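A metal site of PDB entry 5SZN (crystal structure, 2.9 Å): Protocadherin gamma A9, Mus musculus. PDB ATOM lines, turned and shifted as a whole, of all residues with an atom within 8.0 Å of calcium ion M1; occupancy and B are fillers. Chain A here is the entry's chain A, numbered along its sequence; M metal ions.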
ATOM      1  N   GLU A 385     -32.866   0.536  14.547  1.00  0.00           N
ATOM      2  CA  GLU A 385     -32.958   0.082  15.931  1.00  0.00           C
ATOM      3  C   GLU A 385     -33.354   1.208  16.880  1.00  0.00           C
ATOM      4  O   GLU A 385     -33.677   0.925  18.039  1.00  0.00           O
ATOM      5  CB  GLU A 385     -31.647  -0.553  16.376  1.00  0.00           C
ATOM      6  CG  GLU A 385     -31.462  -1.982  15.901  1.00  0.00           C
ATOM      7  CD  GLU A 385     -31.180  -2.085  14.413  1.00  0.00           C
ATOM      8  OE1 GLU A 385     -30.475  -1.215  13.877  1.00  0.00           O
ATOM      9  OE2 GLU A 385     -31.678  -3.048  13.773  1.00  0.00           O
ATOM     10  N   ASP A 416     -33.751  -3.153   6.565  1.00  0.00           N
ATOM     11  CA  ASP A 416     -32.842  -3.731   7.545  1.00  0.00           C
ATOM     12  C   ASP A 416     -31.542  -4.141   6.857  1.00  0.00           C
ATOM     13  O   ASP A 416     -31.547  -5.012   5.981  1.00  0.00           O
ATOM     14  CB  ASP A 416     -33.462  -4.935   8.252  1.00  0.00           C
ATOM     15  CG  ASP A 416     -32.587  -5.486   9.359  1.00  0.00           C
ATOM     16  OD1 ASP A 416     -31.748  -4.731   9.890  1.00  0.00           O
ATOM     17  OD2 ASP A 416     -32.724  -6.682   9.699  1.00  0.00           O
ATOM     18  N   ILE A 417     -30.446  -3.523   7.266  1.00  0.00           N
ATOM     19  CA  ILE A 417     -29.094  -3.918   6.868  1.00  0.00           C
ATOM     20  C   ILE A 417     -28.413  -4.514   8.083  1.00  0.00           C
ATOM     21  O   ILE A 417     -28.450  -3.930   9.176  1.00  0.00           O
ATOM     22  CB  ILE A 417     -28.302  -2.723   6.302  1.00  0.00           C
ATOM     23  CG1 ILE A 417     -28.955  -2.213   5.010  1.00  0.00           C
ATOM     24  CG2 ILE A 417     -26.858  -3.120   6.041  1.00  0.00           C
ATOM     25  CD1 ILE A 417     -29.056  -3.266   3.928  1.00  0.00           C
ATOM     26  N   ASN A 418     -27.791  -5.680   7.904  1.00  0.00           N
ATOM     27  CA  ASN A 418     -27.246  -6.460   9.009  1.00  0.00           C
ATOM     28  C   ASN A 418     -25.927  -5.839   9.472  1.00  0.00           C
ATOM     29  O   ASN A 418     -24.877  -6.051   8.865  1.00  0.00           O
ATOM     30  CB  ASN A 418     -27.049  -7.910   8.583  1.00  0.00           C
ATOM     31  CG  ASN A 418     -26.668  -8.803   9.744  1.00  0.00           C
ATOM     32  OD1 ASN A 418     -26.767  -8.417  10.911  1.00  0.00           O
ATOM     33  ND2 ASN A 418     -26.234 -10.027   9.436  1.00  0.00           N
ATOM     34  N   ASP A 419     -25.985  -5.077  10.561  1.00  0.00           N
ATOM     35  CA  ASP A 419     -24.795  -4.511  11.187  1.00  0.00           C
ATOM     36  C   ASP A 419     -24.756  -4.757  12.684  1.00  0.00           C
ATOM     37  O   ASP A 419     -23.916  -4.168  13.373  1.00  0.00           O
ATOM     38  CB  ASP A 419     -24.705  -3.008  10.894  1.00  0.00           C
ATOM     39  CG  ASP A 419     -25.937  -2.245  11.355  1.00  0.00           C
ATOM     40  OD1 ASP A 419     -27.028  -2.834  11.346  1.00  0.00           O
ATOM     41  OD2 ASP A 419     -25.799  -1.062  11.722  1.00  0.00           O
ATOM     42  N   ASN A 420     -25.625  -5.620  13.216  1.00  0.00           N
ATOM     43  CA  ASN A 420     -25.675  -5.918  14.645  1.00  0.00           C
ATOM     44  C   ASN A 420     -25.498  -7.407  14.860  1.00  0.00           C
ATOM     45  O   ASN A 420     -26.308  -8.204  14.354  1.00  0.00           O
ATOM     46  CB  ASN A 420     -26.992  -5.435  15.246  1.00  0.00           C
ATOM     47  CG  ASN A 420     -27.146  -3.929  15.172  1.00  0.00           C
ATOM     48  OD1 ASN A 420     -26.165  -3.195  15.175  1.00  0.00           O
ATOM     49  ND2 ASN A 420     -28.394  -3.469  15.109  1.00  0.00           N
ATOM     50  N   PRO A 421     -24.486  -7.850  15.599  1.00  0.00           N
ATOM     51  CA  PRO A 421     -24.263  -9.280  15.796  1.00  0.00           C
ATOM     52  C   PRO A 421     -25.154  -9.813  16.905  1.00  0.00           C
ATOM     53  O   PRO A 421     -25.626  -9.053  17.760  1.00  0.00           O
ATOM     54  CB  PRO A 421     -22.790  -9.357  16.189  1.00  0.00           C
ATOM     55  CG  PRO A 421     -22.553  -8.068  16.902  1.00  0.00           C
ATOM     56  CD  PRO A 421     -23.424  -7.038  16.218  1.00  0.00           C
ATOM     57  N   PRO A 422     -25.414 -11.123  16.924  1.00  0.00           N
ATOM     58  CA  PRO A 422     -26.210 -11.693  18.024  1.00  0.00           C
ATOM     59  C   PRO A 422     -25.423 -11.663  19.323  1.00  0.00           C
ATOM     60  O   PRO A 422     -24.202 -11.847  19.349  1.00  0.00           O
ATOM     61  CB  PRO A 422     -26.479 -13.123  17.557  1.00  0.00           C
ATOM     62  CG  PRO A 422     -25.360 -13.428  16.613  1.00  0.00           C
ATOM     63  CD  PRO A 422     -25.048 -12.131  15.916  1.00  0.00           C
ATOM     64  N   ALA A 423     -26.149 -11.431  20.419  1.00  0.00           N
ATOM     65  CA  ALA A 423     -25.555 -11.333  21.747  1.00  0.00           C
ATOM     66  C   ALA A 423     -26.208 -12.324  22.690  1.00  0.00           C
ATOM     67  O   ALA A 423     -27.436 -12.473  22.697  1.00  0.00           O
ATOM     68  CB  ALA A 423     -25.687  -9.911  22.309  1.00  0.00           C
ATOM     69  N   HIS A 449     -29.774 -13.197  21.440  1.00  0.00           N
ATOM     70  CA  HIS A 449     -30.715 -12.269  20.820  1.00  0.00           C
ATOM     71  C   HIS A 449     -29.962 -11.393  19.831  1.00  0.00           C
ATOM     72  O   HIS A 449     -28.777 -11.099  20.009  1.00  0.00           O
ATOM     73  CB  HIS A 449     -31.427 -11.410  21.863  1.00  0.00           C
ATOM     74  CG  HIS A 449     -32.441 -10.470  21.291  1.00  0.00           C
ATOM     75  ND1 HIS A 449     -32.116  -9.204  20.846  1.00  0.00           N
ATOM     76  CD2 HIS A 449     -33.773 -10.608  21.083  1.00  0.00           C
ATOM     77  CE1 HIS A 449     -33.208  -8.606  20.394  1.00  0.00           C
ATOM     78  NE2 HIS A 449     -34.222  -9.439  20.527  1.00  0.00           N
ATOM     79  N   ASP A 450     -30.673 -10.962  18.785  1.00  0.00           N
ATOM     80  CA  ASP A 450     -30.091 -10.141  17.728  1.00  0.00           C
ATOM     81  C   ASP A 450     -30.988  -8.929  17.490  1.00  0.00           C
ATOM     82  O   ASP A 450     -32.204  -9.088  17.311  1.00  0.00           O
ATOM     83  CB  ASP A 450     -29.915 -10.950  16.445  1.00  0.00           C
ATOM     84  CG  ASP A 450     -29.007 -10.262  15.433  1.00  0.00           C
ATOM     85  OD1 ASP A 450     -29.183  -9.055  15.182  1.00  0.00           O
ATOM     86  OD2 ASP A 450     -28.120 -10.947  14.872  1.00  0.00           O
ATOM     87  N   PRO A 451     -30.441  -7.708  17.491  1.00  0.00           N
ATOM     88  CA  PRO A 451     -31.290  -6.532  17.318  1.00  0.00           C
ATOM     89  C   PRO A 451     -31.947  -6.421  15.954  1.00  0.00           C
ATOM     90  O   PRO A 451     -33.012  -5.807  15.844  1.00  0.00           O
ATOM     91  CB  PRO A 451     -30.322  -5.362  17.560  1.00  0.00           C
ATOM     92  CG  PRO A 451     -29.203  -5.948  18.344  1.00  0.00           C
ATOM     93  CD  PRO A 451     -29.052  -7.353  17.851  1.00  0.00           C
ATOM     94  N   ASP A 452     -31.347  -7.001  14.916  1.00  0.00           N
ATOM     95  CA  ASP A 452     -31.887  -6.875  13.559  1.00  0.00           C
ATOM     96  C   ASP A 452     -33.207  -7.644  13.448  1.00  0.00           C
ATOM     97  O   ASP A 452     -33.753  -8.154  14.427  1.00  0.00           O
ATOM     98  CB  ASP A 452     -30.857  -7.365  12.537  1.00  0.00           C
ATOM     99  CG  ASP A 452     -29.669  -6.442  12.419  1.00  0.00           C
ATOM    100  OD1 ASP A 452     -29.819  -5.237  12.724  1.00  0.00           O
ATOM    101  OD2 ASP A 452     -28.590  -6.908  12.020  1.00  0.00           O
ATOM    102  N   ASP A 453     -33.734  -7.724  12.231  1.00  0.00           N
ATOM    103  CA  ASP A 453     -35.037  -8.329  12.005  1.00  0.00           C
ATOM    104  C   ASP A 453     -34.925  -9.460  10.982  1.00  0.00           C
ATOM    105  O   ASP A 453     -34.047  -9.443  10.112  1.00  0.00           O
ATOM    106  CB  ASP A 453     -36.057  -7.295  11.519  1.00  0.00           C
ATOM    107  CG  ASP A 453     -37.477  -7.826  11.531  1.00  0.00           C
ATOM    108  OD1 ASP A 453     -37.710  -8.905  12.127  1.00  0.00           O
ATOM    109  OD2 ASP A 453     -38.370  -7.163  10.965  1.00  0.00           O
ATOM    110  N   GLU A 454     -35.809 -10.443  11.122  1.00  0.00           N
ATOM    111  CA  GLU A 454     -35.930 -11.570  10.201  1.00  0.00           C
ATOM    112  C   GLU A 454     -34.647 -12.405  10.164  1.00  0.00           C
ATOM    113  O   GLU A 454     -34.149 -12.823  11.216  1.00  0.00           O
ATOM    114  CB  GLU A 454     -36.321 -11.071   8.810  1.00  0.00           C
ATOM    115  CG  GLU A 454     -37.582 -10.216   8.757  1.00  0.00           C
ATOM    116  CD  GLU A 454     -38.871 -11.027   8.912  1.00  0.00           C
ATOM    117  OE1 GLU A 454     -38.788 -12.256   9.118  1.00  0.00           O
ATOM    118  OE2 GLU A 454     -39.972 -10.428   8.827  1.00  0.00           O
ATOM    119  N   GLU A 455     -34.112 -12.692   8.979  1.00  0.00           N
ATOM    120  CA  GLU A 455     -33.002 -13.629   8.889  1.00  0.00           C
ATOM    121  C   GLU A 455     -31.769 -13.108   9.614  1.00  0.00           C
ATOM    122  O   GLU A 455     -31.005 -13.890  10.175  1.00  0.00           O
ATOM    123  CB  GLU A 455     -32.665 -13.933   7.424  1.00  0.00           C
ATOM    124  CG  GLU A 455     -32.262 -12.723   6.630  1.00  0.00           C
ATOM    125  CD  GLU A 455     -31.677 -13.073   5.287  1.00  0.00           C
ATOM    126  OE1 GLU A 455     -31.556 -14.274   4.969  1.00  0.00           O
ATOM    127  OE2 GLU A 455     -31.328 -12.127   4.535  1.00  0.00           O
ATOM    128  N   ASN A 456     -31.582 -11.786   9.643  1.00  0.00           N
ATOM    129  CA  ASN A 456     -30.443 -11.193  10.344  1.00  0.00           C
ATOM    130  C   ASN A 456     -30.625 -11.185  11.852  1.00  0.00           C
ATOM    131  O   ASN A 456     -29.831 -10.563  12.573  1.00  0.00           O
ATOM    132  CB  ASN A 456     -30.201  -9.777   9.829  1.00  0.00           C
ATOM    133  CG  ASN A 456     -29.949  -9.747   8.330  1.00  0.00           C
ATOM    134  OD1 ASN A 456     -29.530 -10.734   7.736  1.00  0.00           O
ATOM    135  ND2 ASN A 456     -30.211  -8.590   7.716  1.00  0.00           N
ATOM    136  N   ALA A 457     -31.664 -11.868  12.336  1.00  0.00           N
ATOM    137  CA  ALA A 457     -31.851 -12.135  13.754  1.00  0.00           C
ATOM    138  C   ALA A 457     -32.018 -13.622  14.040  1.00  0.00           C
ATOM    139  O   ALA A 457     -32.438 -13.982  15.150  1.00  0.00           O
ATOM    140  CB  ALA A 457     -33.044 -11.351  14.312  1.00  0.00           C
ATOM    141  N   LYS A 458     -31.725 -14.481  13.068  1.00  0.00           N
ATOM    142  CA  LYS A 458     -31.863 -15.929  13.226  1.00  0.00           C
ATOM    143  C   LYS A 458     -30.528 -16.501  13.683  1.00  0.00           C
ATOM    144  O   LYS A 458     -29.550 -16.493  12.931  1.00  0.00           O
ATOM    145  CB  LYS A 458     -32.324 -16.564  11.914  1.00  0.00           C
ATOM    146  N   SER A 507     -24.349 -17.135  15.005  1.00  0.00           N
ATOM    147  CA  SER A 507     -24.228 -16.421  13.748  1.00  0.00           C
ATOM    148  C   SER A 507     -25.612 -16.210  13.134  1.00  0.00           C
ATOM    149  O   SER A 507     -26.450 -17.117  13.177  1.00  0.00           O
ATOM    150  CB  SER A 507     -23.331 -17.171  12.756  1.00  0.00           C
ATOM    151  OG  SER A 507     -22.015 -17.315  13.253  1.00  0.00           O
ATOM    152  N   ASP A 508     -25.841 -15.018  12.593  1.00  0.00           N
ATOM    153  CA  ASP A 508     -27.096 -14.715  11.929  1.00  0.00           C
ATOM    154  C   ASP A 508     -27.092 -15.285  10.516  1.00  0.00           C
ATOM    155  O   ASP A 508     -26.134 -15.100   9.760  1.00  0.00           O
ATOM    156  CB  ASP A 508     -27.357 -13.209  11.907  1.00  0.00           C
ATOM    157  CG  ASP A 508     -26.092 -12.404  11.648  1.00  0.00           C
ATOM    158  OD1 ASP A 508     -25.105 -12.981  11.168  1.00  0.00           O
ATOM    159  OD2 ASP A 508     -26.105 -11.185  11.940  1.00  0.00           O
ATOM    160  N   ASN A 509     -28.178 -15.978  10.152  1.00  0.00           N
ATOM    161  CA  ASN A 509     -28.225 -16.761   8.911  1.00  0.00           C
ATOM    162  C   ASN A 509     -28.667 -15.860   7.758  1.00  0.00           C
ATOM    163  O   ASN A 509     -29.824 -15.851   7.336  1.00  0.00           O
ATOM    164  CB  ASN A 509     -29.142 -17.967   9.070  1.00  0.00           C
ATOM    165  CG  ASN A 509     -29.111 -18.885   7.873  1.00  0.00           C
ATOM    166  OD1 ASN A 509     -28.322 -18.693   6.936  1.00  0.00           O
ATOM    167  ND2 ASN A 509     -29.963 -19.905   7.889  1.00  0.00           N
ATOM    168  N   GLY A 510     -27.703 -15.117   7.233  1.00  0.00           N
ATOM    169  CA  GLY A 510     -27.886 -14.316   6.041  1.00  0.00           C
ATOM    170  C   GLY A 510     -26.555 -13.727   5.631  1.00  0.00           C
ATOM    171  O   GLY A 510     -25.777 -13.346   6.502  1.00  0.00           O
ATOM    172  N   PRO A 512     -24.134 -10.891   4.331  1.00  0.00           N
ATOM    173  CA  PRO A 512     -23.018 -11.393   5.141  1.00  0.00           C
ATOM    174  C   PRO A 512     -23.405 -11.719   6.587  1.00  0.00           C
ATOM    175  O   PRO A 512     -24.254 -11.040   7.161  1.00  0.00           O
ATOM    176  CB  PRO A 512     -22.029 -10.231   5.102  1.00  0.00           C
ATOM    177  CG  PRO A 512     -22.900  -9.030   5.026  1.00  0.00           C
ATOM    178  CD  PRO A 512     -24.096  -9.421   4.197  1.00  0.00           C
ATOM    179  N   PRO A 513     -22.793 -12.753   7.154  1.00  0.00           N
ATOM    180  CA  PRO A 513     -23.142 -13.167   8.523  1.00  0.00           C
ATOM    181  C   PRO A 513     -22.256 -12.519   9.572  1.00  0.00           C
ATOM    182  O   PRO A 513     -21.104 -12.152   9.338  1.00  0.00           O
ATOM    183  CB  PRO A 513     -22.908 -14.679   8.474  1.00  0.00           C
ATOM    184  CG  PRO A 513     -21.767 -14.839   7.526  1.00  0.00           C
ATOM    185  CD  PRO A 513     -21.893 -13.728   6.508  1.00  0.00           C
ATOM    186  N   LEU A 514     -22.833 -12.369  10.769  1.00  0.00           N
ATOM    187  CA  LEU A 514     -22.145 -11.830  11.925  1.00  0.00           C
ATOM    188  C   LEU A 514     -22.141 -12.860  13.033  1.00  0.00           C
ATOM    189  O   LEU A 514     -23.178 -13.462  13.333  1.00  0.00           O
ATOM    190  CB  LEU A 514     -22.814 -10.531  12.417  1.00  0.00           C
ATOM    191  CG  LEU A 514     -22.417  -9.224  11.718  1.00  0.00           C
ATOM    192  CD1 LEU A 514     -23.005  -9.144  10.312  1.00  0.00           C
ATOM    193  CD2 LEU A 514     -22.849  -8.028  12.550  1.00  0.00           C
ATOM    194  N   SER A 515     -20.973 -13.071  13.645  1.00  0.00           N
ATOM    195  CA  SER A 515     -20.772 -14.146  14.600  1.00  0.00           C
ATOM    196  C   SER A 515     -20.325 -13.602  15.952  1.00  0.00           C
ATOM    197  O   SER A 515     -19.812 -12.489  16.061  1.00  0.00           O
ATOM    198  CB  SER A 515     -19.734 -15.152  14.069  1.00  0.00           C
ATOM    199  OG  SER A 515     -20.148 -15.692  12.821  1.00  0.00           O
HETATM  200 CA    CA M   1     -27.653  -9.630  12.836  1.00  0.00          CA
HETATM  201 CA    CA M   2     -30.371  -3.315  11.369  1.00  0.00          CA
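OD1 of Asp 450 lies close to N of Asp 452.
OD2 of Asp 452 lies close to OD1 of Asn 418 (2.6 Å).
The backbone carbonyl oxygen (O) of Leu 514 sits at hydrogen-bond distance from the backbone NH (N) of Asp 508 (3.2 Å).
The side-chain carboxylate (OD2) of Asp 452 lies within hydrogen-bond range of the backbone NH (N) of Asn 420 (3.4 Å).
The side-chain carboxylate (OE1) of Glu 385 sits close to the side-chain amide nitrogen (ND2) of Asn 420 (3.3 Å).
The side-chain amide nitrogen (ND2) of Asn 418 lies within hydrogen-bond range of the backbone carbonyl oxygen (O) of Pro 512, 3.2 Å away.
Within 4 Å of calcium ion M1: Asn 418, Asn 420, Asp 450, Asp 452, Asn 456 and Asp 508.
The nearest printed residue that does not touch calcium ion M1 is Pro 421 (4.5 Å).
Calcium ion M1 is bound by OD2 of Asp 508 (2.4 Å).
O of Asn 456 binds calcium ion M1, at 2.4 Å.
OD1 of Asn 418 is bound to calcium ion M1.
OD2 of Asp 450 binds calcium ion M1 (2.5 Å).
Calcium ion M1 is bound by O of Asn 420, 2.5 Å away.
OD1 of Asp 450 is bound to calcium ion M1 (2.9 Å).
Calcium ion M1 has six donor atoms within binding distance.
Slightly farther from calcium ion M1 lies the side-chain carboxylate (OD2) of Asp 452 (3.0 Å).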
